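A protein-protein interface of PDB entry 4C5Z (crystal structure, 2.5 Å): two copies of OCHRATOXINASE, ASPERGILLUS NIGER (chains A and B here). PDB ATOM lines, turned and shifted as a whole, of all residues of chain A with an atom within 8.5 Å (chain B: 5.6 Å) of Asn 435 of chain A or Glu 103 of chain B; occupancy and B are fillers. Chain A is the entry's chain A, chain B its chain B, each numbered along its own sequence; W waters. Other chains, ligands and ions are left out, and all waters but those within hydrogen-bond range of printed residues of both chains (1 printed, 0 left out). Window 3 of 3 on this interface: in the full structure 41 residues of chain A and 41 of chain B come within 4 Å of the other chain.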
ATOM      1  N   GLY A 129      11.213   6.635 -13.576  1.00  0.00           N
ATOM      2  CA  GLY A 129      10.899   7.409 -14.769  1.00  0.00           C
ATOM      3  C   GLY A 129      10.654   6.607 -16.019  1.00  0.00           C
ATOM      4  O   GLY A 129      10.392   7.188 -17.067  1.00  0.00           O
ATOM      5  N   THR A 130      10.707   5.285 -15.920  1.00  0.00           N
ATOM      6  CA  THR A 130      10.592   4.408 -17.071  1.00  0.00           C
ATOM      7  C   THR A 130       9.203   4.451 -17.676  1.00  0.00           C
ATOM      8  O   THR A 130       9.043   4.444 -18.906  1.00  0.00           O
ATOM      9  CB  THR A 130      10.936   2.949 -16.684  1.00  0.00           C
ATOM     10  OG1 THR A 130      12.238   2.902 -16.083  1.00  0.00           O
ATOM     11  CG2 THR A 130      10.988   2.054 -17.905  1.00  0.00           C
ATOM     12  N   PRO A 428       3.019  11.845 -24.961  1.00  0.00           N
ATOM     13  CA  PRO A 428       2.410  10.752 -24.222  1.00  0.00           C
ATOM     14  C   PRO A 428       3.099  10.473 -22.899  1.00  0.00           C
ATOM     15  O   PRO A 428       2.440  10.133 -21.940  1.00  0.00           O
ATOM     16  CB  PRO A 428       2.550   9.551 -25.159  1.00  0.00           C
ATOM     17  CG  PRO A 428       2.920  10.095 -26.479  1.00  0.00           C
ATOM     18  CD  PRO A 428       3.509  11.442 -26.281  1.00  0.00           C
ATOM     19  N   TRP A 429       4.414  10.643 -22.829  1.00  0.00           N
ATOM     20  CA  TRP A 429       5.122  10.339 -21.587  1.00  0.00           C
ATOM     21  C   TRP A 429       5.432  11.573 -20.731  1.00  0.00           C
ATOM     22  O   TRP A 429       6.223  11.491 -19.810  1.00  0.00           O
ATOM     23  CB  TRP A 429       6.374   9.517 -21.894  1.00  0.00           C
ATOM     24  CG  TRP A 429       6.005   8.295 -22.658  1.00  0.00           C
ATOM     25  CD1 TRP A 429       6.110   8.109 -24.000  1.00  0.00           C
ATOM     26  CD2 TRP A 429       5.365   7.127 -22.137  1.00  0.00           C
ATOM     27  NE1 TRP A 429       5.603   6.886 -24.340  1.00  0.00           N
ATOM     28  CE2 TRP A 429       5.160   6.254 -23.211  1.00  0.00           C
ATOM     29  CE3 TRP A 429       4.983   6.718 -20.859  1.00  0.00           C
ATOM     30  CZ2 TRP A 429       4.592   4.988 -23.046  1.00  0.00           C
ATOM     31  CZ3 TRP A 429       4.414   5.477 -20.710  1.00  0.00           C
ATOM     32  CH2 TRP A 429       4.211   4.637 -21.793  1.00  0.00           C
ATOM     33  N   ASP A 432       9.285  16.968 -21.383  1.00  0.00           N
ATOM     34  CA  ASP A 432      10.722  16.756 -21.408  1.00  0.00           C
ATOM     35  C   ASP A 432      11.004  15.271 -21.328  1.00  0.00           C
ATOM     36  O   ASP A 432      12.051  14.870 -20.829  1.00  0.00           O
ATOM     37  CB  ASP A 432      11.430  17.512 -20.239  1.00  0.00           C
ATOM     38  CG  ASP A 432      11.074  19.015 -20.181  1.00  0.00           C
ATOM     39  OD1 ASP A 432      11.103  19.689 -21.240  1.00  0.00           O
ATOM     40  OD2 ASP A 432      10.767  19.514 -19.068  1.00  0.00           O
ATOM     41  N   ALA A 433      10.061  14.454 -21.790  1.00  0.00           N
ATOM     42  CA  ALA A 433      10.221  13.010 -21.746  1.00  0.00           C
ATOM     43  C   ALA A 433      11.344  12.603 -22.701  1.00  0.00           C
ATOM     44  O   ALA A 433      11.474  13.155 -23.775  1.00  0.00           O
ATOM     45  CB  ALA A 433       8.924  12.319 -22.112  1.00  0.00           C
ATOM     46  N   ARG A 434      12.187  11.685 -22.242  1.00  0.00           N
ATOM     47  CA  ARG A 434      13.259  11.108 -23.019  1.00  0.00           C
ATOM     48  C   ARG A 434      13.091   9.598 -22.967  1.00  0.00           C
ATOM     49  O   ARG A 434      12.650   9.046 -21.984  1.00  0.00           O
ATOM     50  CB  ARG A 434      14.620  11.497 -22.423  1.00  0.00           C
ATOM     51  CG  ARG A 434      15.213  12.826 -22.907  1.00  0.00           C
ATOM     52  CD  ARG A 434      16.588  13.134 -22.279  1.00  0.00           C
ATOM     53  NE  ARG A 434      17.696  12.258 -22.743  1.00  0.00           N
ATOM     54  CZ  ARG A 434      18.138  11.137 -22.139  1.00  0.00           C
ATOM     55  NH1 ARG A 434      17.587  10.681 -21.005  1.00  0.00           N
ATOM     56  NH2 ARG A 434      19.152  10.454 -22.679  1.00  0.00           N
ATOM     57  N   ASN A 435      13.442   8.930 -24.042  1.00  0.00           N
ATOM     58  CA  ASN A 435      13.483   7.478 -24.058  1.00  0.00           C
ATOM     59  C   ASN A 435      14.506   6.952 -23.040  1.00  0.00           C
ATOM     60  O   ASN A 435      15.725   7.091 -23.260  1.00  0.00           O
ATOM     61  CB  ASN A 435      13.859   7.009 -25.471  1.00  0.00           C
ATOM     62  CG  ASN A 435      14.044   5.510 -25.572  1.00  0.00           C
ATOM     63  OD1 ASN A 435      13.863   4.780 -24.603  1.00  0.00           O
ATOM     64  ND2 ASN A 435      14.389   5.039 -26.766  1.00  0.00           N
ATOM     65  N   PRO A 436      14.037   6.315 -21.946  1.00  0.00           N
ATOM     66  CA  PRO A 436      14.989   5.923 -20.903  1.00  0.00           C
ATOM     67  C   PRO A 436      15.921   4.756 -21.262  1.00  0.00           C
ATOM     68  O   PRO A 436      16.737   4.369 -20.445  1.00  0.00           O
ATOM     69  CB  PRO A 436      14.099   5.547 -19.722  1.00  0.00           C
ATOM     70  CG  PRO A 436      12.725   5.386 -20.265  1.00  0.00           C
ATOM     71  CD  PRO A 436      12.720   5.710 -21.729  1.00  0.00           C
ATOM     72  N   PHE A 437      15.827   4.213 -22.463  1.00  0.00           N
ATOM     73  CA  PHE A 437      16.637   3.054 -22.836  1.00  0.00           C
ATOM     74  C   PHE A 437      17.789   3.431 -23.762  1.00  0.00           C
ATOM     75  O   PHE A 437      18.483   2.570 -24.280  1.00  0.00           O
ATOM     76  CB  PHE A 437      15.719   1.976 -23.434  1.00  0.00           C
ATOM     77  CG  PHE A 437      14.637   1.530 -22.477  1.00  0.00           C
ATOM     78  CD1 PHE A 437      14.948   0.718 -21.390  1.00  0.00           C
ATOM     79  CD2 PHE A 437      13.331   1.962 -22.621  1.00  0.00           C
ATOM     80  CE1 PHE A 437      13.979   0.315 -20.496  1.00  0.00           C
ATOM     81  CE2 PHE A 437      12.352   1.578 -21.725  1.00  0.00           C
ATOM     82  CZ  PHE A 437      12.675   0.747 -20.661  1.00  0.00           C
ATOM     83  N   LEU A 438      17.975   4.732 -23.964  1.00  0.00           N
ATOM     84  CA  LEU A 438      19.097   5.262 -24.747  1.00  0.00           C
ATOM     85  C   LEU A 438      20.119   5.977 -23.854  1.00  0.00           C
ATOM     86  O   LEU A 438      21.323   6.078 -24.176  1.00  0.00           O
ATOM     87  CB  LEU A 438      18.559   6.234 -25.793  1.00  0.00           C
ATOM     88  CG  LEU A 438      17.639   5.629 -26.853  1.00  0.00           C
ATOM     89  CD1 LEU A 438      17.141   6.690 -27.841  1.00  0.00           C
ATOM     90  CD2 LEU A 438      18.353   4.502 -27.589  1.00  0.00           C
ATOM     91  OXT LEU A 438      19.720   6.477 -22.789  1.00  0.00           O
ATOM     92  N   ALA B  98       7.097  -2.521 -21.213  1.00  0.00           N
ATOM     93  CA  ALA B  98       6.006  -1.903 -21.952  1.00  0.00           C
ATOM     94  C   ALA B  98       6.449  -0.576 -22.558  1.00  0.00           C
ATOM     95  O   ALA B  98       6.173  -0.302 -23.711  1.00  0.00           O
ATOM     96  CB  ALA B  98       4.808  -1.696 -21.050  1.00  0.00           C
ATOM     97  N   ARG B  99       7.142   0.253 -21.780  1.00  0.00           N
ATOM     98  CA  ARG B  99       7.715   1.479 -22.344  1.00  0.00           C
ATOM     99  C   ARG B  99       8.623   1.146 -23.529  1.00  0.00           C
ATOM    100  O   ARG B  99       8.603   1.825 -24.557  1.00  0.00           O
ATOM    101  CB  ARG B  99       8.527   2.245 -21.308  1.00  0.00           C
ATOM    102  CG  ARG B  99       9.214   3.487 -21.857  1.00  0.00           C
ATOM    103  CD  ARG B  99       8.172   4.521 -22.222  1.00  0.00           C
ATOM    104  NE  ARG B  99       8.725   5.800 -22.657  1.00  0.00           N
ATOM    105  CZ  ARG B  99       9.162   6.766 -21.857  1.00  0.00           C
ATOM    106  NH1 ARG B  99       9.162   6.592 -20.555  1.00  0.00           N
ATOM    107  NH2 ARG B  99       9.637   7.896 -22.381  1.00  0.00           N
ATOM    108  N   GLY B 100       9.425   0.113 -23.368  1.00  0.00           N
ATOM    109  CA  GLY B 100      10.432  -0.196 -24.343  1.00  0.00           C
ATOM    110  C   GLY B 100       9.841  -0.652 -25.650  1.00  0.00           C
ATOM    111  O   GLY B 100      10.313  -0.243 -26.692  1.00  0.00           O
ATOM    112  N   CYS B 101       8.808  -1.507 -25.590  1.00  0.00           N
ATOM    113  CA  CYS B 101       8.121  -1.976 -26.805  1.00  0.00           C
ATOM    114  C   CYS B 101       7.372  -0.846 -27.540  1.00  0.00           C
ATOM    115  O   CYS B 101       7.295  -0.831 -28.773  1.00  0.00           O
ATOM    116  CB  CYS B 101       7.141  -3.106 -26.489  1.00  0.00           C
ATOM    117  SG  CYS B 101       7.883  -4.642 -25.937  1.00  0.00           S
ATOM    118  N   TRP B 102       6.807   0.084 -26.765  1.00  0.00           N
ATOM    119  CA  TRP B 102       6.207   1.294 -27.327  1.00  0.00           C
ATOM    120  C   TRP B 102       7.260   2.063 -28.097  1.00  0.00           C
ATOM    121  O   TRP B 102       7.041   2.519 -29.199  1.00  0.00           O
ATOM    122  CB  TRP B 102       5.673   2.223 -26.231  1.00  0.00           C
ATOM    123  CG  TRP B 102       4.994   3.376 -26.786  1.00  0.00           C
ATOM    124  CD1 TRP B 102       3.733   3.407 -27.238  1.00  0.00           C
ATOM    125  CD2 TRP B 102       5.540   4.678 -27.017  1.00  0.00           C
ATOM    126  NE1 TRP B 102       3.441   4.635 -27.737  1.00  0.00           N
ATOM    127  CE2 TRP B 102       4.526   5.449 -27.591  1.00  0.00           C
ATOM    128  CE3 TRP B 102       6.800   5.266 -26.812  1.00  0.00           C
ATOM    129  CZ2 TRP B 102       4.710   6.790 -27.959  1.00  0.00           C
ATOM    130  CZ3 TRP B 102       6.978   6.589 -27.174  1.00  0.00           C
ATOM    131  CH2 TRP B 102       5.934   7.338 -27.756  1.00  0.00           C
ATOM    132  N   GLU B 103       8.404   2.222 -27.465  1.00  0.00           N
ATOM    133  CA  GLU B 103       9.470   3.040 -27.980  1.00  0.00           C
ATOM    134  C   GLU B 103      10.046   2.358 -29.215  1.00  0.00           C
ATOM    135  O   GLU B 103      10.353   2.985 -30.217  1.00  0.00           O
ATOM    136  CB  GLU B 103      10.488   3.260 -26.848  1.00  0.00           C
ATOM    137  CG  GLU B 103      11.125   4.627 -26.859  1.00  0.00           C
ATOM    138  CD  GLU B 103      10.318   5.770 -26.265  1.00  0.00           C
ATOM    139  OE1 GLU B 103       9.802   5.691 -25.139  1.00  0.00           O
ATOM    140  OE2 GLU B 103      10.279   6.818 -26.904  1.00  0.00           O
ATOM    141  N   ALA B 104      10.086   1.050 -29.183  1.00  0.00           N
ATOM    142  CA  ALA B 104      10.555   0.283 -30.304  1.00  0.00           C
ATOM    143  C   ALA B 104       9.702   0.548 -31.541  1.00  0.00           C
ATOM    144  O   ALA B 104      10.203   0.725 -32.665  1.00  0.00           O
ATOM    145  CB  ALA B 104      10.495  -1.200 -29.959  1.00  0.00           C
ATOM    146  N   LEU B 105       8.400   0.509 -31.338  1.00  0.00           N
ATOM    147  CA  LEU B 105       7.475   0.665 -32.442  1.00  0.00           C
ATOM    148  C   LEU B 105       7.595   2.077 -33.044  1.00  0.00           C
ATOM    149  O   LEU B 105       7.566   2.252 -34.272  1.00  0.00           O
ATOM    150  CB  LEU B 105       6.051   0.366 -31.969  1.00  0.00           C
ATOM    151  CG  LEU B 105       5.128  -0.360 -32.946  1.00  0.00           C
ATOM    152  CD1 LEU B 105       5.796  -1.491 -33.719  1.00  0.00           C
ATOM    153  CD2 LEU B 105       3.926  -0.869 -32.193  1.00  0.00           C
ATOM    154  N   GLN B 106       7.809   3.062 -32.186  1.00  0.00           N
ATOM    155  CA  GLN B 106       7.973   4.404 -32.658  1.00  0.00           C
ATOM    156  C   GLN B 106       9.219   4.581 -33.534  1.00  0.00           C
ATOM    157  O   GLN B 106       9.247   5.481 -34.348  1.00  0.00           O
ATOM    158  CB  GLN B 106       8.012   5.372 -31.484  1.00  0.00           C
ATOM    159  CG  GLN B 106       6.738   5.385 -30.650  1.00  0.00           C
ATOM    160  CD  GLN B 106       5.639   6.219 -31.269  1.00  0.00           C
ATOM    161  OE1 GLN B 106       5.773   7.428 -31.470  1.00  0.00           O
ATOM    162  NE2 GLN B 106       4.533   5.580 -31.543  1.00  0.00           N
ATOM    163  N   ASN B 107      10.245   3.748 -33.361  1.00  0.00           N
ATOM    164  CA  ASN B 107      11.446   3.797 -34.215  1.00  0.00           C
ATOM    165  C   ASN B 107      11.330   2.934 -35.448  1.00  0.00           C
ATOM    166  O   ASN B 107      12.307   2.811 -36.166  1.00  0.00           O
ATOM    167  CB  ASN B 107      12.712   3.307 -33.506  1.00  0.00           C
ATOM    168  CG  ASN B 107      13.081   4.084 -32.262  1.00  0.00           C
ATOM    169  OD1 ASN B 107      12.498   5.111 -31.931  1.00  0.00           O
ATOM    170  ND2 ASN B 107      14.068   3.541 -31.528  1.00  0.00           N
ATOM    171  N   GLY B 108      10.178   2.313 -35.690  1.00  0.00           N
ATOM    172  CA  GLY B 108       9.997   1.490 -36.882  1.00  0.00           C
ATOM    173  C   GLY B 108      10.477   0.055 -36.743  1.00  0.00           C
ATOM    174  O   GLY B 108      10.683  -0.657 -37.728  1.00  0.00           O
ATOM    175  N   GLY B 340      13.454  -0.828 -26.964  1.00  0.00           N
ATOM    176  CA  GLY B 340      13.591   0.638 -26.983  1.00  0.00           C
ATOM    177  C   GLY B 340      15.025   1.149 -27.008  1.00  0.00           C
ATOM    178  O   GLY B 340      15.287   2.333 -27.172  1.00  0.00           O
ATOM    179  N   GLY B 341      15.977   0.246 -26.843  1.00  0.00           N
ATOM    180  CA  GLY B 341      17.371   0.606 -26.920  1.00  0.00           C
ATOM    181  C   GLY B 341      17.787   0.988 -28.317  1.00  0.00           C
ATOM    182  O   GLY B 341      16.974   1.035 -29.250  1.00  0.00           O
HETATM  183  O   HOH W   1       9.503   9.645 -19.144  1.00  0.00           O
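The backbone carbonyl oxygen (O) of Thr 130 of chain A sits at hydrogen-bond distance from the guanidinium group (NH1) of Arg 99 of chain B, at 2.7 Å.
The backbone carbonyl oxygen (O) of Arg 434 of chain A sits at hydrogen-bond distance from the guanidinium group (NH2) of Arg 99 of chain B.
The backbone carbonyl oxygen (O) of Gly 340 of chain B sits at hydrogen-bond distance from the side-chain amide nitrogen (ND2) of Asn 435 of chain A.
The side-chain amide oxygen of Asn 435 of chain A is in hydrogen-bond range of the backbone NH of Phe 437 of chain A (3.0 Å).
The side-chain carboxylate (OE1) of Glu 103 of chain B lies within salt-bridge range of the guanidinium group (NE) of Arg 99 of chain B, at 2.7 Å.
O of Gly 100 of chain B is in hydrogen-bond range of N of Gly 340 of chain B (3.2 Å).
OD1 of Asn 107 of chain B sits close to O of Glu 103 of chain B (3.5 Å).
NH1 of Arg 99 of chain B touches O of Gly 129 of chain A (3.7 Å).
Trp 429 of chain A touches Arg 99 of chain B (CG to CZ, 3.6 Å).
NE1 of Trp 429 of chain A touches CZ3 of Trp 102 of chain B (3.2 Å).
Asn 435 of chain A touches Glu 103 of chain B (ND2 to CG, 3.3 Å).
Arg 99 of chain B touches Pro 436 of chain A (CZ to CD, 3.7 Å).
Phe 437 of chain A touches Arg 99 of chain B.
CB of Phe 437 of chain A touches C of Gly 340 of chain B, 3.7 Å away.
Phe 437 of chain A touches Gly 341 of chain B.
Leu 438 of chain A touches Gly 340 of chain B (CD2 to O, 3.8 Å).
C of Gly 341 of chain B touches CD2 of Leu 438 of chain A (3.6 Å).
Of chain B, only Glu 103 (3.3 Å) and Gly 340 (2.9 Å) come within 4 Å of Asn 435 of chain A.
Ala 104 of chain B touches none of the printed residues of chain A.
Printed residues of chain B within 4 Å of Gly 129 of chain A: Arg 99.
Of the printed residues of chain B, Pro 436 of chain A touches Arg 99.
Leu 105 of chain B touches none of the printed residues of chain A.
The nearest printed residue of chain A that does not touch Trp 102 of chain B is Pro 428 of chain A (4.04 Å).
Of the 11 printed residues of chain A, 8 touch a printed residue of chain B.
Printed residues of chain A that touch a printed residue of chain B: Gly 129, Thr 130, Trp 429, Arg 434, Asn 435, Pro 436, Phe 437 and Leu 438.
Of the 13 printed residues of chain B, 6 touch a printed residue of chain A.
Hydrophobic or aromatic side chains of chain B within 4 Å of the printed part of chain A: Trp 102.
Among the printed residues, 14 pairs touch across the chains.
No position is printed for both chains.
Of the 14 pairs that touch across the chains among the printed residues, none has its exchanged pair printed and touching as well.
Water W1 bridges O of Gly 129 of chain A (3.3 Å) and NH1 of Arg 99 of chain B (3.4 Å).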
